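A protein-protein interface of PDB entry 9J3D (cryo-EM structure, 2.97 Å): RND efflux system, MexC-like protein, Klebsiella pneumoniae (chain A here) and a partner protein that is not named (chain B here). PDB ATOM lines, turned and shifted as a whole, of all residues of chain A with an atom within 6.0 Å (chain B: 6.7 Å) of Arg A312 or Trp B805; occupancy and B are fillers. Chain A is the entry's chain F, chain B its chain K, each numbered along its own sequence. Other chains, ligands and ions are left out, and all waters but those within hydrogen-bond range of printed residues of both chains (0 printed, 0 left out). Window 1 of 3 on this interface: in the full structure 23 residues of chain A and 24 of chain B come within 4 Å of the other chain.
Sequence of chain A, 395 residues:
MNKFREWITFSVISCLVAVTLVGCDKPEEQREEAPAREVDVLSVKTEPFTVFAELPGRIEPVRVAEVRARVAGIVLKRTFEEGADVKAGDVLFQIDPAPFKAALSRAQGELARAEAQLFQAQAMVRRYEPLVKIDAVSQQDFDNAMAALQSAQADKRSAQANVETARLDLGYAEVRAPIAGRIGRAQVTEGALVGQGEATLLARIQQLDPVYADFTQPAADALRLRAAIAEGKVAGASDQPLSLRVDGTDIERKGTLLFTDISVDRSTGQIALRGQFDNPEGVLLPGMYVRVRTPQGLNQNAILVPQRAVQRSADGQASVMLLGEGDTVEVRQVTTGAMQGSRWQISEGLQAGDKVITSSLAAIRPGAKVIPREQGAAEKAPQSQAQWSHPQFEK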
ATOM      1  N   VAL A 310     -25.693  17.720  33.789  1.00  0.00           N
ATOM      2  CA  VAL A 310     -25.135  19.066  33.719  1.00  0.00           C
ATOM      3  C   VAL A 310     -26.268  20.075  33.836  1.00  0.00           C
ATOM      4  O   VAL A 310     -27.240  20.019  33.076  1.00  0.00           O
ATOM      5  CB  VAL A 310     -24.353  19.273  32.415  1.00  0.00           C
ATOM      6  CG1 VAL A 310     -23.826  20.694  32.334  1.00  0.00           C
ATOM      7  CG2 VAL A 310     -23.215  18.272  32.317  1.00  0.00           C
ATOM      8  N   GLN A 311     -26.150  20.999  34.786  1.00  0.00           N
ATOM      9  CA  GLN A 311     -27.119  22.070  34.953  1.00  0.00           C
ATOM     10  C   GLN A 311     -26.533  23.371  34.422  1.00  0.00           C
ATOM     11  O   GLN A 311     -25.314  23.555  34.420  1.00  0.00           O
ATOM     12  CB  GLN A 311     -27.507  22.236  36.423  1.00  0.00           C
ATOM     13  CG  GLN A 311     -27.580  20.941  37.218  1.00  0.00           C
ATOM     14  CD  GLN A 311     -28.680  20.012  36.745  1.00  0.00           C
ATOM     15  OE1 GLN A 311     -28.577  19.390  35.689  1.00  0.00           O
ATOM     16  NE2 GLN A 311     -29.748  19.920  37.527  1.00  0.00           N
ATOM     17  N   ARG A 312     -27.400  24.264  33.960  1.00  0.00           N
ATOM     18  CA  ARG A 312     -26.982  25.568  33.463  1.00  0.00           C
ATOM     19  C   ARG A 312     -27.733  26.659  34.209  1.00  0.00           C
ATOM     20  O   ARG A 312     -28.957  26.583  34.362  1.00  0.00           O
ATOM     21  CB  ARG A 312     -27.221  25.688  31.958  1.00  0.00           C
ATOM     22  CG  ARG A 312     -26.278  24.841  31.121  1.00  0.00           C
ATOM     23  CD  ARG A 312     -26.267  25.279  29.670  1.00  0.00           C
ATOM     24  NE  ARG A 312     -25.323  24.500  28.881  1.00  0.00           N
ATOM     25  CZ  ARG A 312     -24.057  24.840  28.683  1.00  0.00           C
ATOM     26  NH1 ARG A 312     -23.548  25.941  29.209  1.00  0.00           N
ATOM     27  NH2 ARG A 312     -23.284  24.056  27.938  1.00  0.00           N
ATOM     28  N   SER A 313     -27.000  27.665  34.673  1.00  0.00           N
ATOM     29  CA  SER A 313     -27.594  28.745  35.437  1.00  0.00           C
ATOM     30  C   SER A 313     -28.101  29.845  34.509  1.00  0.00           C
ATOM     31  O   SER A 313     -28.012  29.757  33.282  1.00  0.00           O
ATOM     32  CB  SER A 313     -26.584  29.311  36.433  1.00  0.00           C
ATOM     33  OG  SER A 313     -25.289  29.368  35.862  1.00  0.00           O
ATOM     34  N   ALA A 314     -28.643  30.902  35.120  1.00  0.00           N
ATOM     35  CA  ALA A 314     -29.208  32.005  34.354  1.00  0.00           C
ATOM     36  C   ALA A 314     -28.159  32.740  33.534  1.00  0.00           C
ATOM     37  O   ALA A 314     -28.501  33.363  32.523  1.00  0.00           O
ATOM     38  CB  ALA A 314     -29.918  32.986  35.288  1.00  0.00           C
ATOM     39  N   ASP A 315     -26.895  32.687  33.941  1.00  0.00           N
ATOM     40  CA  ASP A 315     -25.822  33.320  33.187  1.00  0.00           C
ATOM     41  C   ASP A 315     -25.240  32.410  32.116  1.00  0.00           C
ATOM     42  O   ASP A 315     -24.292  32.812  31.433  1.00  0.00           O
ATOM     43  CB  ASP A 315     -24.710  33.772  34.134  1.00  0.00           C
ATOM     44  CG  ASP A 315     -24.197  32.645  35.008  1.00  0.00           C
ATOM     45  OD1 ASP A 315     -24.821  31.564  35.015  1.00  0.00           O
ATOM     46  OD2 ASP A 315     -23.168  32.838  35.688  1.00  0.00           O
ATOM     47  N   GLY A 316     -25.775  31.203  31.955  1.00  0.00           N
ATOM     48  CA  GLY A 316     -25.244  30.250  31.008  1.00  0.00           C
ATOM     49  C   GLY A 316     -24.093  29.414  31.518  1.00  0.00           C
ATOM     50  O   GLY A 316     -23.610  28.545  30.781  1.00  0.00           O
ATOM     51  N   GLN A 317     -23.639  29.644  32.746  1.00  0.00           N
ATOM     52  CA  GLN A 317     -22.539  28.867  33.298  1.00  0.00           C
ATOM     53  C   GLN A 317     -23.003  27.460  33.648  1.00  0.00           C
ATOM     54  O   GLN A 317     -24.092  27.264  34.193  1.00  0.00           O
ATOM     55  CB  GLN A 317     -21.974  29.562  34.536  1.00  0.00           C
ATOM     56  CG  GLN A 317     -21.256  28.651  35.521  1.00  0.00           C
ATOM     57  CD  GLN A 317     -19.911  28.162  35.011  1.00  0.00           C
ATOM     58  OE1 GLN A 317     -19.809  27.597  33.923  1.00  0.00           O
ATOM     59  NE2 GLN A 317     -18.866  28.395  35.796  1.00  0.00           N
ATOM     60  N   ALA A 318     -22.166  26.476  33.331  1.00  0.00           N
ATOM     61  CA  ALA A 318     -22.499  25.078  33.560  1.00  0.00           C
ATOM     62  C   ALA A 318     -21.933  24.603  34.891  1.00  0.00           C
ATOM     63  O   ALA A 318     -20.828  24.984  35.284  1.00  0.00           O
ATOM     64  CB  ALA A 318     -21.967  24.204  32.425  1.00  0.00           C
ATOM     65  N   SER A 319     -22.691  23.750  35.573  1.00  0.00           N
ATOM     66  CA  SER A 319     -22.301  23.231  36.871  1.00  0.00           C
ATOM     67  C   SER A 319     -22.767  21.789  37.003  1.00  0.00           C
ATOM     68  O   SER A 319     -23.622  21.316  36.248  1.00  0.00           O
ATOM     69  CB  SER A 319     -22.878  24.079  38.010  1.00  0.00           C
ATOM     70  OG  SER A 319     -24.293  24.050  37.998  1.00  0.00           O
ATOM     71  N   THR A 336     -18.046  22.910  29.575  1.00  0.00           N
ATOM     72  CA  THR A 336     -18.384  21.825  28.667  1.00  0.00           C
ATOM     73  C   THR A 336     -17.631  21.989  27.355  1.00  0.00           C
ATOM     74  O   THR A 336     -17.497  23.104  26.844  1.00  0.00           O
ATOM     75  CB  THR A 336     -19.888  21.791  28.410  1.00  0.00           C
ATOM     76  OG1 THR A 336     -20.308  23.051  27.875  1.00  0.00           O
ATOM     77  CG2 THR A 336     -20.637  21.527  29.700  1.00  0.00           C
ATOM     78  N   TRP A 344     -21.599  14.962  27.582  1.00  0.00           N
ATOM     79  CA  TRP A 344     -20.806  16.173  27.489  1.00  0.00           C
ATOM     80  C   TRP A 344     -19.351  15.874  27.816  1.00  0.00           C
ATOM     81  O   TRP A 344     -19.046  15.176  28.789  1.00  0.00           O
ATOM     82  CB  TRP A 344     -21.337  17.229  28.461  1.00  0.00           C
ATOM     83  CG  TRP A 344     -22.193  18.295  27.853  1.00  0.00           C
ATOM     84  CD1 TRP A 344     -23.454  18.639  28.232  1.00  0.00           C
ATOM     85  CD2 TRP A 344     -21.841  19.176  26.785  1.00  0.00           C
ATOM     86  NE1 TRP A 344     -23.918  19.670  27.457  1.00  0.00           N
ATOM     87  CE2 TRP A 344     -22.944  20.019  26.560  1.00  0.00           C
ATOM     88  CE3 TRP A 344     -20.704  19.330  25.991  1.00  0.00           C
ATOM     89  CZ2 TRP A 344     -22.944  21.000  25.576  1.00  0.00           C
ATOM     90  CZ3 TRP A 344     -20.706  20.303  25.014  1.00  0.00           C
ATOM     91  CH2 TRP A 344     -21.817  21.125  24.814  1.00  0.00           C
ATOM     92  N   ALA B 720     -35.549  27.371  30.790  1.00  0.00           N
ATOM     93  CA  ALA B 720     -34.711  26.363  30.169  1.00  0.00           C
ATOM     94  C   ALA B 720     -33.497  27.005  29.513  1.00  0.00           C
ATOM     95  O   ALA B 720     -33.541  28.182  29.127  1.00  0.00           O
ATOM     96  CB  ALA B 720     -35.501  25.565  29.122  1.00  0.00           C
ATOM     97  N   PRO B 721     -32.393  26.270  29.396  1.00  0.00           N
ATOM     98  CA  PRO B 721     -31.236  26.787  28.655  1.00  0.00           C
ATOM     99  C   PRO B 721     -31.549  27.049  27.192  1.00  0.00           C
ATOM    100  O   PRO B 721     -32.288  26.294  26.553  1.00  0.00           O
ATOM    101  CB  PRO B 721     -30.195  25.673  28.812  1.00  0.00           C
ATOM    102  CG  PRO B 721     -30.586  24.967  30.059  1.00  0.00           C
ATOM    103  CD  PRO B 721     -32.081  25.014  30.099  1.00  0.00           C
ATOM    104  N   GLN B 722     -30.977  28.121  26.657  1.00  0.00           N
ATOM    105  CA  GLN B 722     -31.091  28.487  25.256  1.00  0.00           C
ATOM    106  C   GLN B 722     -29.697  28.679  24.679  1.00  0.00           C
ATOM    107  O   GLN B 722     -28.756  29.011  25.407  1.00  0.00           O
ATOM    108  CB  GLN B 722     -31.914  29.767  25.084  1.00  0.00           C
ATOM    109  CG  GLN B 722     -33.333  29.668  25.612  1.00  0.00           C
ATOM    110  CD  GLN B 722     -34.135  30.928  25.363  1.00  0.00           C
ATOM    111  OE1 GLN B 722     -33.613  31.917  24.851  1.00  0.00           O
ATOM    112  NE2 GLN B 722     -35.412  30.895  25.720  1.00  0.00           N
ATOM    113  N   LEU B 723     -29.564  28.459  23.375  1.00  0.00           N
ATOM    114  CA  LEU B 723     -28.271  28.548  22.700  1.00  0.00           C
ATOM    115  C   LEU B 723     -28.289  29.755  21.773  1.00  0.00           C
ATOM    116  O   LEU B 723     -28.593  29.634  20.586  1.00  0.00           O
ATOM    117  CB  LEU B 723     -27.978  27.263  21.936  1.00  0.00           C
ATOM    118  CG  LEU B 723     -26.625  27.187  21.232  1.00  0.00           C
ATOM    119  CD1 LEU B 723     -25.506  27.109  22.247  1.00  0.00           C
ATOM    120  CD2 LEU B 723     -26.579  25.998  20.289  1.00  0.00           C
ATOM    121  N   ARG B 724     -27.950  30.922  22.310  1.00  0.00           N
ATOM    122  CA  ARG B 724     -27.942  32.147  21.525  1.00  0.00           C
ATOM    123  C   ARG B 724     -26.884  32.063  20.435  1.00  0.00           C
ATOM    124  O   ARG B 724     -25.758  31.616  20.680  1.00  0.00           O
ATOM    125  CB  ARG B 724     -27.680  33.349  22.430  1.00  0.00           C
ATOM    126  CG  ARG B 724     -26.944  34.496  21.762  1.00  0.00           C
ATOM    127  CD  ARG B 724     -27.899  35.594  21.351  1.00  0.00           C
ATOM    128  NE  ARG B 724     -28.876  35.874  22.394  1.00  0.00           N
ATOM    129  CZ  ARG B 724     -29.699  36.913  22.388  1.00  0.00           C
ATOM    130  NH1 ARG B 724     -29.691  37.794  21.401  1.00  0.00           N
ATOM    131  NH2 ARG B 724     -30.554  37.069  23.394  1.00  0.00           N
ATOM    132  N   PRO B 779     -25.293  20.882  18.880  1.00  0.00           N
ATOM    133  CA  PRO B 779     -24.992  22.279  18.527  1.00  0.00           C
ATOM    134  C   PRO B 779     -23.955  22.423  17.428  1.00  0.00           C
ATOM    135  O   PRO B 779     -23.994  23.404  16.676  1.00  0.00           O
ATOM    136  CB  PRO B 779     -24.497  22.870  19.853  1.00  0.00           C
ATOM    137  CG  PRO B 779     -25.131  22.028  20.894  1.00  0.00           C
ATOM    138  CD  PRO B 779     -25.165  20.643  20.327  1.00  0.00           C
ATOM    139  N   THR B 803     -21.789  30.252  19.122  1.00  0.00           N
ATOM    140  CA  THR B 803     -22.855  29.768  19.986  1.00  0.00           C
ATOM    141  C   THR B 803     -22.503  30.029  21.443  1.00  0.00           C
ATOM    142  O   THR B 803     -21.394  29.715  21.886  1.00  0.00           O
ATOM    143  CB  THR B 803     -23.099  28.273  19.773  1.00  0.00           C
ATOM    144  OG1 THR B 803     -21.924  27.542  20.138  1.00  0.00           O
ATOM    145  CG2 THR B 803     -23.430  27.991  18.320  1.00  0.00           C
ATOM    146  N   SER B 804     -23.445  30.610  22.183  1.00  0.00           N
ATOM    147  CA  SER B 804     -23.242  30.883  23.600  1.00  0.00           C
ATOM    148  C   SER B 804     -24.487  30.480  24.370  1.00  0.00           C
ATOM    149  O   SER B 804     -25.602  30.803  23.960  1.00  0.00           O
ATOM    150  CB  SER B 804     -22.929  32.363  23.842  1.00  0.00           C
ATOM    151  OG  SER B 804     -23.961  33.190  23.338  1.00  0.00           O
ATOM    152  N   TRP B 805     -24.298  29.791  25.490  1.00  0.00           N
ATOM    153  CA  TRP B 805     -25.430  29.317  26.272  1.00  0.00           C
ATOM    154  C   TRP B 805     -25.899  30.395  27.240  1.00  0.00           C
ATOM    155  O   TRP B 805     -25.085  31.048  27.901  1.00  0.00           O
ATOM    156  CB  TRP B 805     -25.058  28.048  27.035  1.00  0.00           C
ATOM    157  CG  TRP B 805     -24.920  26.840  26.167  1.00  0.00           C
ATOM    158  CD1 TRP B 805     -23.771  26.341  25.635  1.00  0.00           C
ATOM    159  CD2 TRP B 805     -25.973  25.976  25.731  1.00  0.00           C
ATOM    160  NE1 TRP B 805     -24.041  25.218  24.893  1.00  0.00           N
ATOM    161  CE2 TRP B 805     -25.388  24.973  24.938  1.00  0.00           C
ATOM    162  CE3 TRP B 805     -27.353  25.953  25.934  1.00  0.00           C
ATOM    163  CZ2 TRP B 805     -26.134  23.961  24.346  1.00  0.00           C
ATOM    164  CZ3 TRP B 805     -28.092  24.946  25.348  1.00  0.00           C
ATOM    165  CH2 TRP B 805     -27.482  23.964  24.563  1.00  0.00           C
ATOM    166  N   GLU B 806     -27.213  30.584  27.313  1.00  0.00           N
ATOM    167  CA  GLU B 806     -27.846  31.408  28.332  1.00  0.00           C
ATOM    168  C   GLU B 806     -29.119  30.705  28.779  1.00  0.00           C
ATOM    169  O   GLU B 806     -29.327  29.529  28.486  1.00  0.00           O
ATOM    170  CB  GLU B 806     -28.153  32.823  27.824  1.00  0.00           C
ATOM    171  CG  GLU B 806     -29.056  32.883  26.611  1.00  0.00           C
ATOM    172  CD  GLU B 806     -29.051  34.250  25.952  1.00  0.00           C
ATOM    173  OE1 GLU B 806     -28.188  35.078  26.307  1.00  0.00           O
ATOM    174  OE2 GLU B 806     -29.911  34.498  25.080  1.00  0.00           O
ATOM    175  N   GLU B 807     -29.978  31.420  29.495  1.00  0.00           N
ATOM    176  CA  GLU B 807     -31.236  30.848  29.947  1.00  0.00           C
ATOM    177  C   GLU B 807     -32.404  31.740  29.549  1.00  0.00           C
ATOM    178  O   GLU B 807     -32.296  32.968  29.545  1.00  0.00           O
ATOM    179  CB  GLU B 807     -31.231  30.636  31.462  1.00  0.00           C
ATOM    180  CG  GLU B 807     -32.418  29.842  31.978  1.00  0.00           C
ATOM    181  CD  GLU B 807     -32.161  29.219  33.335  1.00  0.00           C
ATOM    182  OE1 GLU B 807     -31.040  29.375  33.859  1.00  0.00           O
ATOM    183  OE2 GLU B 807     -33.080  28.572  33.878  1.00  0.00           O
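CG of Pro B721 touches CB of Arg A312, 3.9 Å away.
Arg A312 touches Glu B807.
CA of Gly A316 touches O of Trp B805 (3.2 Å).
CA of Glu B806 touches CA of Gly A316, at 3.9 Å.
NH1 of Arg A312 lies within hydrogen-bond range of O of Gly A316, at 3.0 Å.
The guanidinium group of Arg A312 lies within hydrogen-bond range of the side-chain hydroxyl of Thr A336 (3.1 Å).
The side-chain carboxylate (OD1) of Asp A315 sits at hydrogen-bond distance from the side-chain hydroxyl (OG) of Ser A313, 2.4 Å away.
The backbone carbonyl oxygen of Gln A317 is in hydrogen-bond range of the side-chain hydroxyl of Ser A313 (2.9 Å).
The backbone NH of Gln B722 is in hydrogen-bond range of the backbone carbonyl oxygen of Glu B806 (2.8 Å).
OE2 of Glu B806 lies within salt-bridge range of NH2 of Arg B724 (3.1 Å).
The backbone NH (N) of Ala A314 is in hydrogen-bond range of the side-chain carboxylate (OE1) of Glu B807 (3.1 Å).
NH2 of Arg A312 sits close to NE1 of Trp B805.
The backbone carbonyl oxygen (O) of Ser A313 sits close to the side-chain carboxylate (OE1) of Glu B807.
Arg A312 touches just these residues of chain B: Pro B721 (3.9 Å), Trp B805 (3.3 Å) and Glu B807 (3.5 Å).
Of the printed residues of chain B, Ser A313 touches Glu B807 (3.0 Å).
Printed residues of chain B within 4 Å of Ala A314: Glu B807 (3.1 Å).
Printed residues of chain B within 4 Å of Gly A316: Trp B805 (3.2 Å) and Glu B806 (3.9 Å).
Of the printed residues of chain A, Pro B721 touches Arg A312.
Leu B723 touches none of the printed residues of chain A.
Trp B805 touches just these residues of chain A: Arg A312 and Gly A316.
Printed residues of chain A within 4 Å of Glu B807: Arg A312, Ser A313 and Ala A314.
The nearest printed residue of chain B that does not touch Gly A316 is Glu B807 (4.9 Å).
Printed residues of chain A that touch a printed residue of chain B: Arg A312, Ser A313, Ala A314 and Gly A316.
Printed residues of chain B that touch a printed residue of chain A: Pro B721, Trp B805, Glu B806 and Glu B807.
Hydrophobic or aromatic side chains of chain B that line the printed part of chain A: Pro B721 and Trp B805.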
